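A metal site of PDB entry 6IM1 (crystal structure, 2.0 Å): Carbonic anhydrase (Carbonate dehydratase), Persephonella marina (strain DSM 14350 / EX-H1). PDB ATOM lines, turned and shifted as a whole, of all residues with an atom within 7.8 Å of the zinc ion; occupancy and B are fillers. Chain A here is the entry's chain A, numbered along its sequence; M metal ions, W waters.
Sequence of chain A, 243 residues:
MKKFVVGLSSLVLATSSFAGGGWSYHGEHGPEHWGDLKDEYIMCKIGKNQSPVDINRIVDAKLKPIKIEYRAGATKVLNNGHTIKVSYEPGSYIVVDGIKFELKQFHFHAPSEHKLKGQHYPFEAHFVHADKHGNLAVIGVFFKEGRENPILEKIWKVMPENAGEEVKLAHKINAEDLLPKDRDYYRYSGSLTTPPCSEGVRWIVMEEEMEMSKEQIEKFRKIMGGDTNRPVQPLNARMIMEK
The zinc ion is bound by water W1, a ring nitrogen (NE2) of His 107, a ring nitrogen (ND1) of His 126 and a ring nitrogen (NE2) of His 109. The zinc ion has four donor atoms within binding distance.
Glu 113 touches the zinc ion (OE1 to ZN, 3.8 Å). OG1 of Thr 193 touches the zinc ion, 3.8 Å away.
A ring nitrogen (ND1) of His 107 sits at hydrogen-bond distance from the side-chain amide oxygen of Gln 105 (2.7 Å). A ring nitrogen (NE2) of His 126 is in hydrogen-bond range of the side-chain carboxylate (OE2) of Glu 124 (2.6 Å). OE1 of Glu 113 sits close to NE2 of His 109 (3.1 Å). The backbone NH of His 109 sits at hydrogen-bond distance from the backbone carbonyl oxygen of Glu 124. O of Thr 228 lies within hydrogen-bond range of ND1 of His 109, 2.7 Å away. The side-chain hydroxyl of Thr 193 lies within hydrogen-bond range of the side-chain carboxylate of Glu 113 (2.5 Å). N of Glu 113 is in hydrogen-bond range of OE1 of Glu 124 (2.7 Å).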
ATOM      1  N   TYR A  25     -12.810  15.433 -14.600  1.00  0.00           N
ATOM      2  CA  TYR A  25     -12.273  15.364 -13.234  1.00  0.00           C
ATOM      3  C   TYR A  25     -10.780  15.011 -13.147  1.00  0.00           C
ATOM      4  O   TYR A  25     -10.217  15.017 -12.059  1.00  0.00           O
ATOM      5  CB  TYR A  25     -13.090  14.338 -12.422  1.00  0.00           C
ATOM      6  CG  TYR A  25     -14.413  14.896 -12.004  1.00  0.00           C
ATOM      7  CD1 TYR A  25     -14.464  16.029 -11.160  1.00  0.00           C
ATOM      8  CD2 TYR A  25     -15.582  14.375 -12.481  1.00  0.00           C
ATOM      9  CE1 TYR A  25     -15.672  16.592 -10.787  1.00  0.00           C
ATOM     10  CE2 TYR A  25     -16.835  14.925 -12.071  1.00  0.00           C
ATOM     11  CZ  TYR A  25     -16.864  16.025 -11.236  1.00  0.00           C
ATOM     12  OH  TYR A  25     -18.064  16.583 -10.818  1.00  0.00           O
ATOM     13  N   THR A  83     -21.669  12.093 -13.531  1.00  0.00           N
ATOM     14  CA  THR A  83     -22.414  11.646 -12.370  1.00  0.00           C
ATOM     15  C   THR A  83     -23.627  10.814 -12.846  1.00  0.00           C
ATOM     16  O   THR A  83     -23.821  10.643 -14.060  1.00  0.00           O
ATOM     17  CB  THR A  83     -22.929  12.897 -11.580  1.00  0.00           C
ATOM     18  OG1 THR A  83     -23.535  12.495 -10.343  1.00  0.00           O
ATOM     19  CG2 THR A  83     -23.981  13.692 -12.398  1.00  0.00           C
ATOM     20  N   GLN A 105     -33.564  18.071  -9.692  1.00  0.00           N
ATOM     21  CA  GLN A 105     -32.805  16.873  -9.890  1.00  0.00           C
ATOM     22  C   GLN A 105     -31.903  16.627  -8.652  1.00  0.00           C
ATOM     23  O   GLN A 105     -31.648  17.562  -7.886  1.00  0.00           O
ATOM     24  CB  GLN A 105     -31.926  16.923 -11.121  1.00  0.00           C
ATOM     25  CG  GLN A 105     -30.998  18.135 -11.322  1.00  0.00           C
ATOM     26  CD  GLN A 105     -29.537  17.934 -10.902  1.00  0.00           C
ATOM     27  OE1 GLN A 105     -29.151  17.005 -10.159  1.00  0.00           O
ATOM     28  NE2 GLN A 105     -28.742  18.859 -11.299  1.00  0.00           N
ATOM     29  N   PHE A 106     -31.465  15.397  -8.515  1.00  0.00           N
ATOM     30  CA  PHE A 106     -30.379  15.074  -7.547  1.00  0.00           C
ATOM     31  C   PHE A 106     -29.320  14.200  -8.191  1.00  0.00           C
ATOM     32  O   PHE A 106     -29.626  13.460  -9.125  1.00  0.00           O
ATOM     33  CB  PHE A 106     -30.932  14.590  -6.210  1.00  0.00           C
ATOM     34  CG  PHE A 106     -31.722  13.310  -6.240  1.00  0.00           C
ATOM     35  CD1 PHE A 106     -31.118  12.119  -6.030  1.00  0.00           C
ATOM     36  CD2 PHE A 106     -33.103  13.345  -6.424  1.00  0.00           C
ATOM     37  CE1 PHE A 106     -31.833  10.917  -6.023  1.00  0.00           C
ATOM     38  CE2 PHE A 106     -33.847  12.174  -6.390  1.00  0.00           C
ATOM     39  CZ  PHE A 106     -33.212  10.954  -6.184  1.00  0.00           C
ATOM     40  N   HIS A 107     -28.087  14.298  -7.726  1.00  0.00           N
ATOM     41  CA  HIS A 107     -27.015  13.572  -8.310  1.00  0.00           C
ATOM     42  C   HIS A 107     -25.957  13.338  -7.252  1.00  0.00           C
ATOM     43  O   HIS A 107     -26.124  13.776  -6.098  1.00  0.00           O
ATOM     44  CB  HIS A 107     -26.459  14.314  -9.510  1.00  0.00           C
ATOM     45  CG  HIS A 107     -25.884  15.632  -9.173  1.00  0.00           C
ATOM     46  ND1 HIS A 107     -26.561  16.833  -9.257  1.00  0.00           N
ATOM     47  CD2 HIS A 107     -24.650  15.938  -8.644  1.00  0.00           C
ATOM     48  CE1 HIS A 107     -25.790  17.862  -8.845  1.00  0.00           C
ATOM     49  NE2 HIS A 107     -24.649  17.297  -8.484  1.00  0.00           N
ATOM     50  N   PHE A 108     -24.896  12.624  -7.624  1.00  0.00           N
ATOM     51  CA  PHE A 108     -23.958  12.092  -6.632  1.00  0.00           C
ATOM     52  C   PHE A 108     -22.500  12.335  -6.976  1.00  0.00           C
ATOM     53  O   PHE A 108     -22.115  12.558  -8.145  1.00  0.00           O
ATOM     54  CB  PHE A 108     -24.218  10.575  -6.520  1.00  0.00           C
ATOM     55  CG  PHE A 108     -25.601  10.256  -6.281  1.00  0.00           C
ATOM     56  CD1 PHE A 108     -26.174  10.401  -5.022  1.00  0.00           C
ATOM     57  CD2 PHE A 108     -26.391   9.781  -7.305  1.00  0.00           C
ATOM     58  CE1 PHE A 108     -27.493  10.071  -4.804  1.00  0.00           C
ATOM     59  CE2 PHE A 108     -27.716   9.483  -7.085  1.00  0.00           C
ATOM     60  CZ  PHE A 108     -28.271   9.625  -5.863  1.00  0.00           C
ATOM     61  N   HIS A 109     -21.682  12.299  -5.937  1.00  0.00           N
ATOM     62  CA  HIS A 109     -20.251  12.396  -6.078  1.00  0.00           C
ATOM     63  C   HIS A 109     -19.523  11.435  -5.139  1.00  0.00           C
ATOM     64  O   HIS A 109     -20.029  11.153  -4.041  1.00  0.00           O
ATOM     65  CB  HIS A 109     -19.790  13.812  -5.689  1.00  0.00           C
ATOM     66  CG  HIS A 109     -20.340  14.876  -6.520  1.00  0.00           C
ATOM     67  ND1 HIS A 109     -19.753  15.315  -7.704  1.00  0.00           N
ATOM     68  CD2 HIS A 109     -21.443  15.665  -6.321  1.00  0.00           C
ATOM     69  CE1 HIS A 109     -20.459  16.325  -8.211  1.00  0.00           C
ATOM     70  NE2 HIS A 109     -21.476  16.505  -7.396  1.00  0.00           N
ATOM     71  N   GLU A 113     -17.608  15.911  -1.965  1.00  0.00           N
ATOM     72  CA  GLU A 113     -17.033  17.203  -2.454  1.00  0.00           C
ATOM     73  C   GLU A 113     -16.635  18.070  -1.298  1.00  0.00           C
ATOM     74  O   GLU A 113     -15.498  18.480  -1.201  1.00  0.00           O
ATOM     75  CB  GLU A 113     -18.012  17.920  -3.366  1.00  0.00           C
ATOM     76  CG  GLU A 113     -18.235  17.100  -4.648  1.00  0.00           C
ATOM     77  CD  GLU A 113     -18.405  17.962  -5.894  1.00  0.00           C
ATOM     78  OE1 GLU A 113     -19.499  18.514  -6.060  1.00  0.00           O
ATOM     79  OE2 GLU A 113     -17.431  18.058  -6.659  1.00  0.00           O
ATOM     80  N   GLU A 124     -21.367  11.716  -1.439  1.00  0.00           N
ATOM     81  CA  GLU A 124     -22.168  12.915  -1.202  1.00  0.00           C
ATOM     82  C   GLU A 124     -23.267  13.034  -2.270  1.00  0.00           C
ATOM     83  O   GLU A 124     -22.995  12.905  -3.479  1.00  0.00           O
ATOM     84  CB  GLU A 124     -21.294  14.193  -1.250  1.00  0.00           C
ATOM     85  CG  GLU A 124     -21.994  15.499  -0.877  1.00  0.00           C
ATOM     86  CD  GLU A 124     -21.042  16.723  -0.747  1.00  0.00           C
ATOM     87  OE1 GLU A 124     -19.836  16.547  -0.484  1.00  0.00           O
ATOM     88  OE2 GLU A 124     -21.489  17.901  -0.906  1.00  0.00           O
ATOM     89  N   ALA A 125     -24.472  13.348  -1.828  1.00  0.00           N
ATOM     90  CA  ALA A 125     -25.605  13.637  -2.700  1.00  0.00           C
ATOM     91  C   ALA A 125     -25.924  15.108  -2.748  1.00  0.00           C
ATOM     92  O   ALA A 125     -25.909  15.780  -1.730  1.00  0.00           O
ATOM     93  CB  ALA A 125     -26.836  12.871  -2.276  1.00  0.00           C
ATOM     94  N   HIS A 126     -26.283  15.591  -3.936  1.00  0.00           N
ATOM     95  CA  HIS A 126     -26.695  16.993  -4.133  1.00  0.00           C
ATOM     96  C   HIS A 126     -28.092  17.065  -4.669  1.00  0.00           C
ATOM     97  O   HIS A 126     -28.374  16.461  -5.702  1.00  0.00           O
ATOM     98  CB  HIS A 126     -25.738  17.727  -5.081  1.00  0.00           C
ATOM     99  CG  HIS A 126     -24.394  17.924  -4.521  1.00  0.00           C
ATOM    100  ND1 HIS A 126     -23.307  18.220  -5.302  1.00  0.00           N
ATOM    101  CD2 HIS A 126     -23.939  17.898  -3.251  1.00  0.00           C
ATOM    102  CE1 HIS A 126     -22.230  18.343  -4.535  1.00  0.00           C
ATOM    103  NE2 HIS A 126     -22.598  18.167  -3.267  1.00  0.00           N
ATOM    104  N   PHE A 127     -28.959  17.806  -3.982  1.00  0.00           N
ATOM    105  CA  PHE A 127     -30.322  18.039  -4.385  1.00  0.00           C
ATOM    106  C   PHE A 127     -30.451  19.452  -4.912  1.00  0.00           C
ATOM    107  O   PHE A 127     -30.318  20.389  -4.122  1.00  0.00           O
ATOM    108  CB  PHE A 127     -31.298  17.772  -3.241  1.00  0.00           C
ATOM    109  CG  PHE A 127     -31.191  16.371  -2.678  1.00  0.00           C
ATOM    110  CD1 PHE A 127     -30.186  16.033  -1.814  1.00  0.00           C
ATOM    111  CD2 PHE A 127     -32.069  15.397  -3.085  1.00  0.00           C
ATOM    112  CE1 PHE A 127     -30.014  14.723  -1.353  1.00  0.00           C
ATOM    113  CE2 PHE A 127     -31.921  14.118  -2.637  1.00  0.00           C
ATOM    114  CZ  PHE A 127     -30.876  13.768  -1.794  1.00  0.00           C
ATOM    115  N   VAL A 128     -30.601  19.589  -6.211  1.00  0.00           N
ATOM    116  CA  VAL A 128     -30.571  20.869  -6.875  1.00  0.00           C
ATOM    117  C   VAL A 128     -31.923  21.492  -7.107  1.00  0.00           C
ATOM    118  O   VAL A 128     -32.766  20.942  -7.734  1.00  0.00           O
ATOM    119  CB  VAL A 128     -29.828  20.782  -8.206  1.00  0.00           C
ATOM    120  CG1 VAL A 128     -29.674  22.131  -8.850  1.00  0.00           C
ATOM    121  CG2 VAL A 128     -28.483  20.118  -8.047  1.00  0.00           C
ATOM    122  N   VAL A 138     -28.851  24.356  -3.239  1.00  0.00           N
ATOM    123  CA  VAL A 138     -28.434  22.986  -3.184  1.00  0.00           C
ATOM    124  C   VAL A 138     -28.314  22.434  -1.779  1.00  0.00           C
ATOM    125  O   VAL A 138     -27.737  23.048  -0.932  1.00  0.00           O
ATOM    126  CB  VAL A 138     -27.109  22.740  -3.938  1.00  0.00           C
ATOM    127  CG1 VAL A 138     -26.849  21.264  -4.092  1.00  0.00           C
ATOM    128  CG2 VAL A 138     -27.111  23.418  -5.273  1.00  0.00           C
ATOM    129  N   ILE A 139     -28.888  21.271  -1.579  1.00  0.00           N
ATOM    130  CA  ILE A 139     -28.822  20.545  -0.358  1.00  0.00           C
ATOM    131  C   ILE A 139     -27.851  19.419  -0.601  1.00  0.00           C
ATOM    132  O   ILE A 139     -27.987  18.637  -1.506  1.00  0.00           O
ATOM    133  CB  ILE A 139     -30.147  19.981   0.130  1.00  0.00           C
ATOM    134  CG1 ILE A 139     -31.109  21.083   0.500  1.00  0.00           C
ATOM    135  CG2 ILE A 139     -29.917  19.094   1.328  1.00  0.00           C
ATOM    136  CD1 ILE A 139     -32.413  20.611   1.020  1.00  0.00           C
ATOM    137  N   LEU A 192     -21.847  26.509  -8.152  1.00  0.00           N
ATOM    138  CA  LEU A 192     -21.913  25.157  -8.771  1.00  0.00           C
ATOM    139  C   LEU A 192     -20.533  24.521  -8.702  1.00  0.00           C
ATOM    140  O   LEU A 192     -19.509  25.227  -8.822  1.00  0.00           O
ATOM    141  CB  LEU A 192     -22.338  25.261 -10.243  1.00  0.00           C
ATOM    142  CG  LEU A 192     -23.729  25.840 -10.441  1.00  0.00           C
ATOM    143  CD1 LEU A 192     -23.999  26.019 -11.946  1.00  0.00           C
ATOM    144  CD2 LEU A 192     -24.768  24.946  -9.834  1.00  0.00           C
ATOM    145  N   THR A 193     -20.462  23.215  -8.499  1.00  0.00           N
ATOM    146  CA  THR A 193     -19.156  22.516  -8.401  1.00  0.00           C
ATOM    147  C   THR A 193     -18.638  21.937  -9.726  1.00  0.00           C
ATOM    148  O   THR A 193     -17.588  21.342  -9.773  1.00  0.00           O
ATOM    149  CB  THR A 193     -19.153  21.428  -7.354  1.00  0.00           C
ATOM    150  OG1 THR A 193     -20.001  20.322  -7.740  1.00  0.00           O
ATOM    151  CG2 THR A 193     -19.625  21.988  -5.996  1.00  0.00           C
ATOM    152  N   THR A 194     -19.372  22.214 -10.795  1.00  0.00           N
ATOM    153  CA  THR A 194     -18.975  21.819 -12.142  1.00  0.00           C
ATOM    154  C   THR A 194     -19.129  22.999 -13.044  1.00  0.00           C
ATOM    155  O   THR A 194     -19.976  23.863 -12.769  1.00  0.00           O
ATOM    156  CB  THR A 194     -19.901  20.721 -12.702  1.00  0.00           C
ATOM    157  OG1 THR A 194     -21.248  21.163 -12.587  1.00  0.00           O
ATOM    158  CG2 THR A 194     -19.782  19.496 -11.883  1.00  0.00           C
ATOM    159  N   TRP A 203     -25.919  27.130  -0.447  1.00  0.00           N
ATOM    160  CA  TRP A 203     -25.564  25.806  -0.022  1.00  0.00           C
ATOM    161  C   TRP A 203     -26.062  25.492   1.362  1.00  0.00           C
ATOM    162  O   TRP A 203     -25.892  26.249   2.306  1.00  0.00           O
ATOM    163  CB  TRP A 203     -24.028  25.553  -0.054  1.00  0.00           C
ATOM    164  CG  TRP A 203     -23.548  25.216  -1.385  1.00  0.00           C
ATOM    165  CD1 TRP A 203     -23.066  26.074  -2.336  1.00  0.00           C
ATOM    166  CD2 TRP A 203     -23.572  23.923  -1.980  1.00  0.00           C
ATOM    167  NE1 TRP A 203     -22.738  25.372  -3.456  1.00  0.00           N
ATOM    168  CE2 TRP A 203     -23.109  24.069  -3.316  1.00  0.00           C
ATOM    169  CE3 TRP A 203     -23.929  22.671  -1.539  1.00  0.00           C
ATOM    170  CZ2 TRP A 203     -22.949  22.996  -4.177  1.00  0.00           C
ATOM    171  CZ3 TRP A 203     -23.820  21.604  -2.374  1.00  0.00           C
ATOM    172  CH2 TRP A 203     -23.289  21.768  -3.662  1.00  0.00           C
ATOM    173  N   THR A 228     -15.125  11.617  -8.564  1.00  0.00           N
ATOM    174  CA  THR A 228     -15.963  12.607  -9.194  1.00  0.00           C
ATOM    175  C   THR A 228     -16.156  13.846  -8.307  1.00  0.00           C
ATOM    176  O   THR A 228     -17.229  14.427  -8.302  1.00  0.00           O
ATOM    177  CB  THR A 228     -17.335  12.011  -9.559  1.00  0.00           C
ATOM    178  OG1 THR A 228     -17.836  11.262  -8.448  1.00  0.00           O
ATOM    179  CG2 THR A 228     -17.195  11.074 -10.812  1.00  0.00           C
HETATM  180 ZN    ZN M   1     -23.008  18.043  -7.428  1.00  0.00          ZN
HETATM  181  O   HOH W   1     -22.145  19.629  -8.381  1.00  0.00           O
